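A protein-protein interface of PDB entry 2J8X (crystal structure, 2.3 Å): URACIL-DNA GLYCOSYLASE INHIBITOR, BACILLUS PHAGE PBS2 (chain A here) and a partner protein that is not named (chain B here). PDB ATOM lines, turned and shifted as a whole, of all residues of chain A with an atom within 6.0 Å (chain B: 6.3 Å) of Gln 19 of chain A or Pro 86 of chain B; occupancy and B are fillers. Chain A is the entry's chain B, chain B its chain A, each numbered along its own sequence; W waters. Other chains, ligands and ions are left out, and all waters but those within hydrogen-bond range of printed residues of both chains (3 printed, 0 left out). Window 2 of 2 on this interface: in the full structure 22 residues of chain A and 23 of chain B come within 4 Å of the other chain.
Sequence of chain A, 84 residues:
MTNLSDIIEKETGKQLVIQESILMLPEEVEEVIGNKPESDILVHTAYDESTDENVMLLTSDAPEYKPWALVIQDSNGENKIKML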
ATOM      1  N   VAL A  17       2.472 -34.402   0.754  1.00  0.00           N
ATOM      2  CA  VAL A  17       3.204 -33.281   1.309  1.00  0.00           C
ATOM      3  C   VAL A  17       3.220 -33.422   2.828  1.00  0.00           C
ATOM      4  O   VAL A  17       2.200 -33.750   3.434  1.00  0.00           O
ATOM      5  CB  VAL A  17       2.546 -31.938   0.909  1.00  0.00           C
ATOM      6  CG1 VAL A  17       2.873 -30.848   1.915  1.00  0.00           C
ATOM      7  CG2 VAL A  17       2.974 -31.530  -0.493  1.00  0.00           C
ATOM      8  N   ILE A  18       4.378 -33.199   3.440  1.00  0.00           N
ATOM      9  CA  ILE A  18       4.454 -33.135   4.898  1.00  0.00           C
ATOM     10  C   ILE A  18       3.658 -31.927   5.379  1.00  0.00           C
ATOM     11  O   ILE A  18       3.894 -30.801   4.948  1.00  0.00           O
ATOM     12  CB  ILE A  18       5.916 -33.049   5.389  1.00  0.00           C
ATOM     13  CG1 ILE A  18       6.633 -34.374   5.114  1.00  0.00           C
ATOM     14  CG2 ILE A  18       5.973 -32.690   6.882  1.00  0.00           C
ATOM     15  CD1 ILE A  18       8.111 -34.347   5.402  1.00  0.00           C
ATOM     16  N   GLN A  19       2.690 -32.172   6.249  1.00  0.00           N
ATOM     17  CA  GLN A  19       1.799 -31.115   6.704  1.00  0.00           C
ATOM     18  C   GLN A  19       2.279 -30.543   8.032  1.00  0.00           C
ATOM     19  O   GLN A  19       2.130 -29.347   8.294  1.00  0.00           O
ATOM     20  CB  GLN A  19       0.359 -31.633   6.775  1.00  0.00           C
ATOM     21  CG  GLN A  19      -0.156 -32.062   5.401  1.00  0.00           C
ATOM     22  CD  GLN A  19      -1.549 -32.669   5.416  1.00  0.00           C
ATOM     23  OE1 GLN A  19      -2.396 -32.321   4.591  1.00  0.00           O
ATOM     24  NE2 GLN A  19      -1.786 -33.594   6.336  1.00  0.00           N
ATOM     25  N   GLU A  20       2.890 -31.393   8.852  1.00  0.00           N
ATOM     26  CA  GLU A  20       3.489 -30.946  10.108  1.00  0.00           C
ATOM     27  C   GLU A  20       4.687 -31.804  10.482  1.00  0.00           C
ATOM     28  O   GLU A  20       4.780 -32.974  10.096  1.00  0.00           O
ATOM     29  CB  GLU A  20       2.464 -30.970  11.246  1.00  0.00           C
ATOM     30  CG  GLU A  20       2.038 -32.373  11.655  1.00  0.00           C
ATOM     31  CD  GLU A  20       0.835 -32.373  12.577  1.00  0.00           C
ATOM     32  OE1 GLU A  20       0.008 -31.442  12.481  1.00  0.00           O
ATOM     33  OE2 GLU A  20       0.716 -33.308  13.397  1.00  0.00           O
ATOM     34  N   SER A  21       5.600 -31.201  11.234  1.00  0.00           N
ATOM     35  CA  SER A  21       6.742 -31.892  11.801  1.00  0.00           C
ATOM     36  C   SER A  21       6.779 -31.610  13.307  1.00  0.00           C
ATOM     37  O   SER A  21       7.167 -30.528  13.738  1.00  0.00           O
ATOM     38  CB  SER A  21       8.026 -31.422  11.121  1.00  0.00           C
ATOM     39  OG  SER A  21       7.955 -31.629   9.711  1.00  0.00           O
ATOM     40  N   THR A  45       4.316 -35.725   9.553  1.00  0.00           N
ATOM     41  CA  THR A  45       3.074 -36.427   9.275  1.00  0.00           C
ATOM     42  C   THR A  45       2.241 -35.817   8.154  1.00  0.00           C
ATOM     43  O   THR A  45       2.186 -34.599   7.968  1.00  0.00           O
ATOM     44  CB  THR A  45       2.238 -36.659  10.568  1.00  0.00           C
ATOM     45  OG1 THR A  45       0.856 -36.861  10.230  1.00  0.00           O
ATOM     46  CG2 THR A  45       2.362 -35.495  11.491  1.00  0.00           C
ATOM     47  N   ALA A  46       1.607 -36.702   7.398  1.00  0.00           N
ATOM     48  CA  ALA A  46       0.773 -36.321   6.280  1.00  0.00           C
ATOM     49  C   ALA A  46      -0.464 -37.195   6.307  1.00  0.00           C
ATOM     50  O   ALA A  46      -0.403 -38.362   6.685  1.00  0.00           O
ATOM     51  CB  ALA A  46       1.526 -36.505   4.971  1.00  0.00           C
ATOM     52  N   TYR A  47      -1.589 -36.615   5.922  1.00  0.00           N
ATOM     53  CA  TYR A  47      -2.824 -37.354   5.789  1.00  0.00           C
ATOM     54  C   TYR A  47      -2.952 -37.844   4.353  1.00  0.00           C
ATOM     55  O   TYR A  47      -2.740 -37.082   3.412  1.00  0.00           O
ATOM     56  CB  TYR A  47      -3.996 -36.450   6.153  1.00  0.00           C
ATOM     57  CG  TYR A  47      -5.351 -37.107   6.079  1.00  0.00           C
ATOM     58  CD1 TYR A  47      -5.721 -38.092   6.990  1.00  0.00           C
ATOM     59  CD2 TYR A  47      -6.271 -36.726   5.110  1.00  0.00           C
ATOM     60  CE1 TYR A  47      -6.966 -38.689   6.925  1.00  0.00           C
ATOM     61  CE2 TYR A  47      -7.517 -37.314   5.039  1.00  0.00           C
ATOM     62  CZ  TYR A  47      -7.861 -38.294   5.945  1.00  0.00           C
ATOM     63  OH  TYR A  47      -9.104 -38.878   5.867  1.00  0.00           O
ATOM     64  N   TYR B  69       4.735 -23.919  10.668  1.00  0.00           N
ATOM     65  CA  TYR B  69       4.688 -24.841   9.547  1.00  0.00           C
ATOM     66  C   TYR B  69       5.714 -24.395   8.505  1.00  0.00           C
ATOM     67  O   TYR B  69       5.902 -23.201   8.300  1.00  0.00           O
ATOM     68  CB  TYR B  69       3.284 -24.869   8.939  1.00  0.00           C
ATOM     69  CG  TYR B  69       2.214 -25.382   9.880  1.00  0.00           C
ATOM     70  CD1 TYR B  69       1.206 -24.544  10.347  1.00  0.00           C
ATOM     71  CD2 TYR B  69       2.216 -26.705  10.306  1.00  0.00           C
ATOM     72  CE1 TYR B  69       0.224 -25.015  11.208  1.00  0.00           C
ATOM     73  CE2 TYR B  69       1.249 -27.183  11.166  1.00  0.00           C
ATOM     74  CZ  TYR B  69       0.256 -26.337  11.615  1.00  0.00           C
ATOM     75  OH  TYR B  69      -0.703 -26.823  12.468  1.00  0.00           O
ATOM     76  N   HIS B  70       6.360 -25.356   7.847  1.00  0.00           N
ATOM     77  CA  HIS B  70       7.517 -25.076   6.987  1.00  0.00           C
ATOM     78  C   HIS B  70       7.249 -25.280   5.491  1.00  0.00           C
ATOM     79  O   HIS B  70       8.186 -25.286   4.681  1.00  0.00           O
ATOM     80  CB  HIS B  70       8.722 -25.928   7.423  1.00  0.00           C
ATOM     81  CG  HIS B  70       8.425 -27.394   7.506  1.00  0.00           C
ATOM     82  ND1 HIS B  70       8.340 -28.204   6.393  1.00  0.00           N
ATOM     83  CD2 HIS B  70       8.189 -28.197   8.571  1.00  0.00           C
ATOM     84  CE1 HIS B  70       8.062 -29.439   6.769  1.00  0.00           C
ATOM     85  NE2 HIS B  70       7.961 -29.462   8.085  1.00  0.00           N
ATOM     86  N   GLN B  73       2.220 -22.946   4.858  1.00  0.00           N
ATOM     87  CA  GLN B  73       0.892 -22.947   5.470  1.00  0.00           C
ATOM     88  C   GLN B  73       0.767 -22.097   6.749  1.00  0.00           C
ATOM     89  O   GLN B  73      -0.342 -21.734   7.148  1.00  0.00           O
ATOM     90  CB  GLN B  73       0.399 -24.386   5.680  1.00  0.00           C
ATOM     91  CG  GLN B  73       1.352 -25.285   6.429  1.00  0.00           C
ATOM     92  CD  GLN B  73       2.446 -25.887   5.561  1.00  0.00           C
ATOM     93  OE1 GLN B  73       3.586 -25.428   5.590  1.00  0.00           O
ATOM     94  NE2 GLN B  73       2.112 -26.934   4.810  1.00  0.00           N
ATOM     95  N   VAL B  81      -3.608 -22.820  10.104  1.00  0.00           N
ATOM     96  CA  VAL B  81      -3.041 -22.669   8.754  1.00  0.00           C
ATOM     97  C   VAL B  81      -3.741 -21.576   7.941  1.00  0.00           C
ATOM     98  O   VAL B  81      -4.920 -21.278   8.151  1.00  0.00           O
ATOM     99  CB  VAL B  81      -3.062 -23.988   7.918  1.00  0.00           C
ATOM    100  CG1 VAL B  81      -2.147 -25.046   8.539  1.00  0.00           C
ATOM    101  CG2 VAL B  81      -4.485 -24.505   7.736  1.00  0.00           C
ATOM    102  N   ALA B  82      -3.001 -20.995   7.001  1.00  0.00           N
ATOM    103  CA  ALA B  82      -3.539 -19.985   6.107  1.00  0.00           C
ATOM    104  C   ALA B  82      -4.619 -20.561   5.197  1.00  0.00           C
ATOM    105  O   ALA B  82      -4.704 -21.776   4.989  1.00  0.00           O
ATOM    106  CB  ALA B  82      -2.421 -19.371   5.283  1.00  0.00           C
ATOM    107  N   GLY B  84      -6.862 -22.068   2.413  1.00  0.00           N
ATOM    108  CA  GLY B  84      -6.626 -22.926   1.261  1.00  0.00           C
ATOM    109  C   GLY B  84      -5.792 -24.162   1.528  1.00  0.00           C
ATOM    110  O   GLY B  84      -5.765 -25.078   0.710  1.00  0.00           O
ATOM    111  N   PHE B  85      -5.103 -24.195   2.667  1.00  0.00           N
ATOM    112  CA  PHE B  85      -4.317 -25.370   3.035  1.00  0.00           C
ATOM    113  C   PHE B  85      -5.166 -26.382   3.787  1.00  0.00           C
ATOM    114  O   PHE B  85      -6.092 -26.001   4.506  1.00  0.00           O
ATOM    115  CB  PHE B  85      -3.087 -24.979   3.859  1.00  0.00           C
ATOM    116  CG  PHE B  85      -2.057 -24.217   3.076  1.00  0.00           C
ATOM    117  CD1 PHE B  85      -2.008 -22.836   3.133  1.00  0.00           C
ATOM    118  CD2 PHE B  85      -1.145 -24.883   2.270  1.00  0.00           C
ATOM    119  CE1 PHE B  85      -1.063 -22.130   2.408  1.00  0.00           C
ATOM    120  CE2 PHE B  85      -0.199 -24.186   1.544  1.00  0.00           C
ATOM    121  CZ  PHE B  85      -0.157 -22.806   1.614  1.00  0.00           C
ATOM    122  N   PRO B  86      -4.864 -27.682   3.609  1.00  0.00           N
ATOM    123  CA  PRO B  86      -5.556 -28.721   4.367  1.00  0.00           C
ATOM    124  C   PRO B  86      -5.383 -28.516   5.865  1.00  0.00           C
ATOM    125  O   PRO B  86      -4.340 -28.025   6.304  1.00  0.00           O
ATOM    126  CB  PRO B  86      -4.844 -30.014   3.942  1.00  0.00           C
ATOM    127  CG  PRO B  86      -4.193 -29.693   2.620  1.00  0.00           C
ATOM    128  CD  PRO B  86      -3.863 -28.232   2.670  1.00  0.00           C
ATOM    129  N   VAL B  87      -6.405 -28.875   6.636  1.00  0.00           N
ATOM    130  CA  VAL B  87      -6.300 -28.896   8.086  1.00  0.00           C
ATOM    131  C   VAL B  87      -5.304 -29.983   8.475  1.00  0.00           C
ATOM    132  O   VAL B  87      -5.510 -31.157   8.166  1.00  0.00           O
ATOM    133  CB  VAL B  87      -7.660 -29.197   8.754  1.00  0.00           C
ATOM    134  CG1 VAL B  87      -7.500 -29.290  10.260  1.00  0.00           C
ATOM    135  CG2 VAL B  87      -8.693 -28.129   8.380  1.00  0.00           C
ATOM    136  N   PRO B  88      -4.215 -29.591   9.150  1.00  0.00           N
ATOM    137  CA  PRO B  88      -3.155 -30.535   9.473  1.00  0.00           C
ATOM    138  C   PRO B  88      -3.578 -31.549  10.545  1.00  0.00           C
ATOM    139  O   PRO B  88      -4.513 -31.293  11.302  1.00  0.00           O
ATOM    140  CB  PRO B  88      -2.020 -29.635   9.974  1.00  0.00           C
ATOM    141  CG  PRO B  88      -2.684 -28.397  10.440  1.00  0.00           C
ATOM    142  CD  PRO B  88      -3.939 -28.231   9.648  1.00  0.00           C
ATOM    143  N   PRO B  89      -2.886 -32.698  10.602  1.00  0.00           N
ATOM    144  CA  PRO B  89      -3.200 -33.815  11.501  1.00  0.00           C
ATOM    145  C   PRO B  89      -3.434 -33.435  12.974  1.00  0.00           C
ATOM    146  O   PRO B  89      -4.431 -33.855  13.560  1.00  0.00           O
ATOM    147  CB  PRO B  89      -1.977 -34.725  11.347  1.00  0.00           C
ATOM    148  CG  PRO B  89      -1.533 -34.478   9.936  1.00  0.00           C
ATOM    149  CD  PRO B  89      -1.718 -32.997   9.752  1.00  0.00           C
ATOM    150  N   ARG B  92      -6.659 -31.358  13.213  1.00  0.00           N
ATOM    151  CA  ARG B  92      -7.757 -32.305  13.059  1.00  0.00           C
ATOM    152  C   ARG B  92      -8.041 -32.994  14.391  1.00  0.00           C
ATOM    153  O   ARG B  92      -9.193 -33.211  14.757  1.00  0.00           O
ATOM    154  CB  ARG B  92      -7.418 -33.352  11.992  1.00  0.00           C
ATOM    155  CG  ARG B  92      -7.356 -32.816  10.561  1.00  0.00           C
ATOM    156  CD  ARG B  92      -6.994 -33.914   9.550  1.00  0.00           C
ATOM    157  NE  ARG B  92      -7.539 -35.211   9.945  1.00  0.00           N
ATOM    158  CZ  ARG B  92      -8.819 -35.553   9.843  1.00  0.00           C
ATOM    159  NH1 ARG B  92      -9.702 -34.696   9.346  1.00  0.00           N
ATOM    160  NH2 ARG B  92      -9.221 -36.756  10.235  1.00  0.00           N
ATOM    161  N   GLY B 111      -8.724 -24.173   8.761  1.00  0.00           N
ATOM    162  CA  GLY B 111      -7.813 -24.140   9.900  1.00  0.00           C
ATOM    163  C   GLY B 111      -7.506 -22.738  10.397  1.00  0.00           C
ATOM    164  O   GLY B 111      -6.430 -22.487  10.945  1.00  0.00           O
HETATM  165  O   HOH W   1       0.317 -27.644   7.663  1.00  0.00           O
HETATM  166  O   HOH W   2       0.284 -29.301  13.849  1.00  0.00           O
HETATM  167  O   HOH W   3       4.943 -28.112   8.052  1.00  0.00           O
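Among the printed residues, pairs that only touch across the chains: Ile 18 of chain A with His 70 of chain B (3.9 Å), Gln 19 of chain A with Tyr 69 of chain B (3.3 Å), Gln 19 of chain A with Pro 86 of chain B (3.4 Å), Gln 19 of chain A with Pro 89 of chain B (3.5 Å), Glu 20 of chain A with Tyr 69 of chain B (3.98 Å), Glu 20 of chain A with Pro 88 of chain B (3.7 Å), Glu 20 of chain A with Pro 89 of chain B (3.6 Å) and Thr 45 of chain A with Pro 89 of chain B (3.4 Å).
Printed residues of chain B within 4 Å of Ile 18 of chain A: His 70.
Of chain B, only Tyr 69, Pro 86 and Pro 89 come within 4 Å of Gln 19 of chain A.
Of the printed residues of chain B, Glu 20 of chain A touches Tyr 69, Pro 88 and Pro 89.
Printed residues of chain B within 4 Å of Thr 45 of chain A: Pro 89.
Phe 85 of chain B touches none of the printed residues of chain A.
Of chain A, only Gln 19 comes within 4 Å of Pro 86 of chain B.
The nearest printed residue of chain A that does not touch Pro 86 of chain B is Tyr 47 of chain A (6.9 Å).
The nearest printed residue of chain B that does not touch Thr 45 of chain A is Pro 88 of chain B (6.8 Å).
Water W2 lies within hydrogen-bond range of the side-chain carboxylate (OE1) of Glu 20 of chain A and the side-chain hydroxyl (OH) of Tyr 69 of chain B.
Water W1 lies within hydrogen-bond range of the backbone carbonyl oxygen (O) of Gln 19 of chain A (2.6 Å) and the side-chain amide nitrogen (NE2) of Gln 73 of chain B (3.4 Å).
Water W3 lies within hydrogen-bond range of O of Gln 19 of chain A and N of His 70 of chain B.
The backbone carbonyl oxygen of Glu 20 of chain A is in hydrogen-bond range of the backbone NH of Thr 45 of chain A (2.8 Å).
The backbone NH (N) of Gln 19 of chain A lies within hydrogen-bond range of the backbone carbonyl oxygen (O) of Thr 45 of chain A, 3.0 Å away.
NE2 of Gln 19 of chain A lies close to N of Tyr 47 of chain A.
OG of Ser 21 of chain A lies within hydrogen-bond range of NE2 of His 70 of chain B (2.7 Å).
Hydrophobic or aromatic side chains of chain A within 4 Å of the printed part of chain B: Ile 18.
Along chain A the printed residues that touch a printed residue of chain B span positions 18 to 45.
Among the printed residues, no Asp or Glu carboxylate lies within 4 Å of a Lys or Arg side-chain nitrogen of the other chain.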
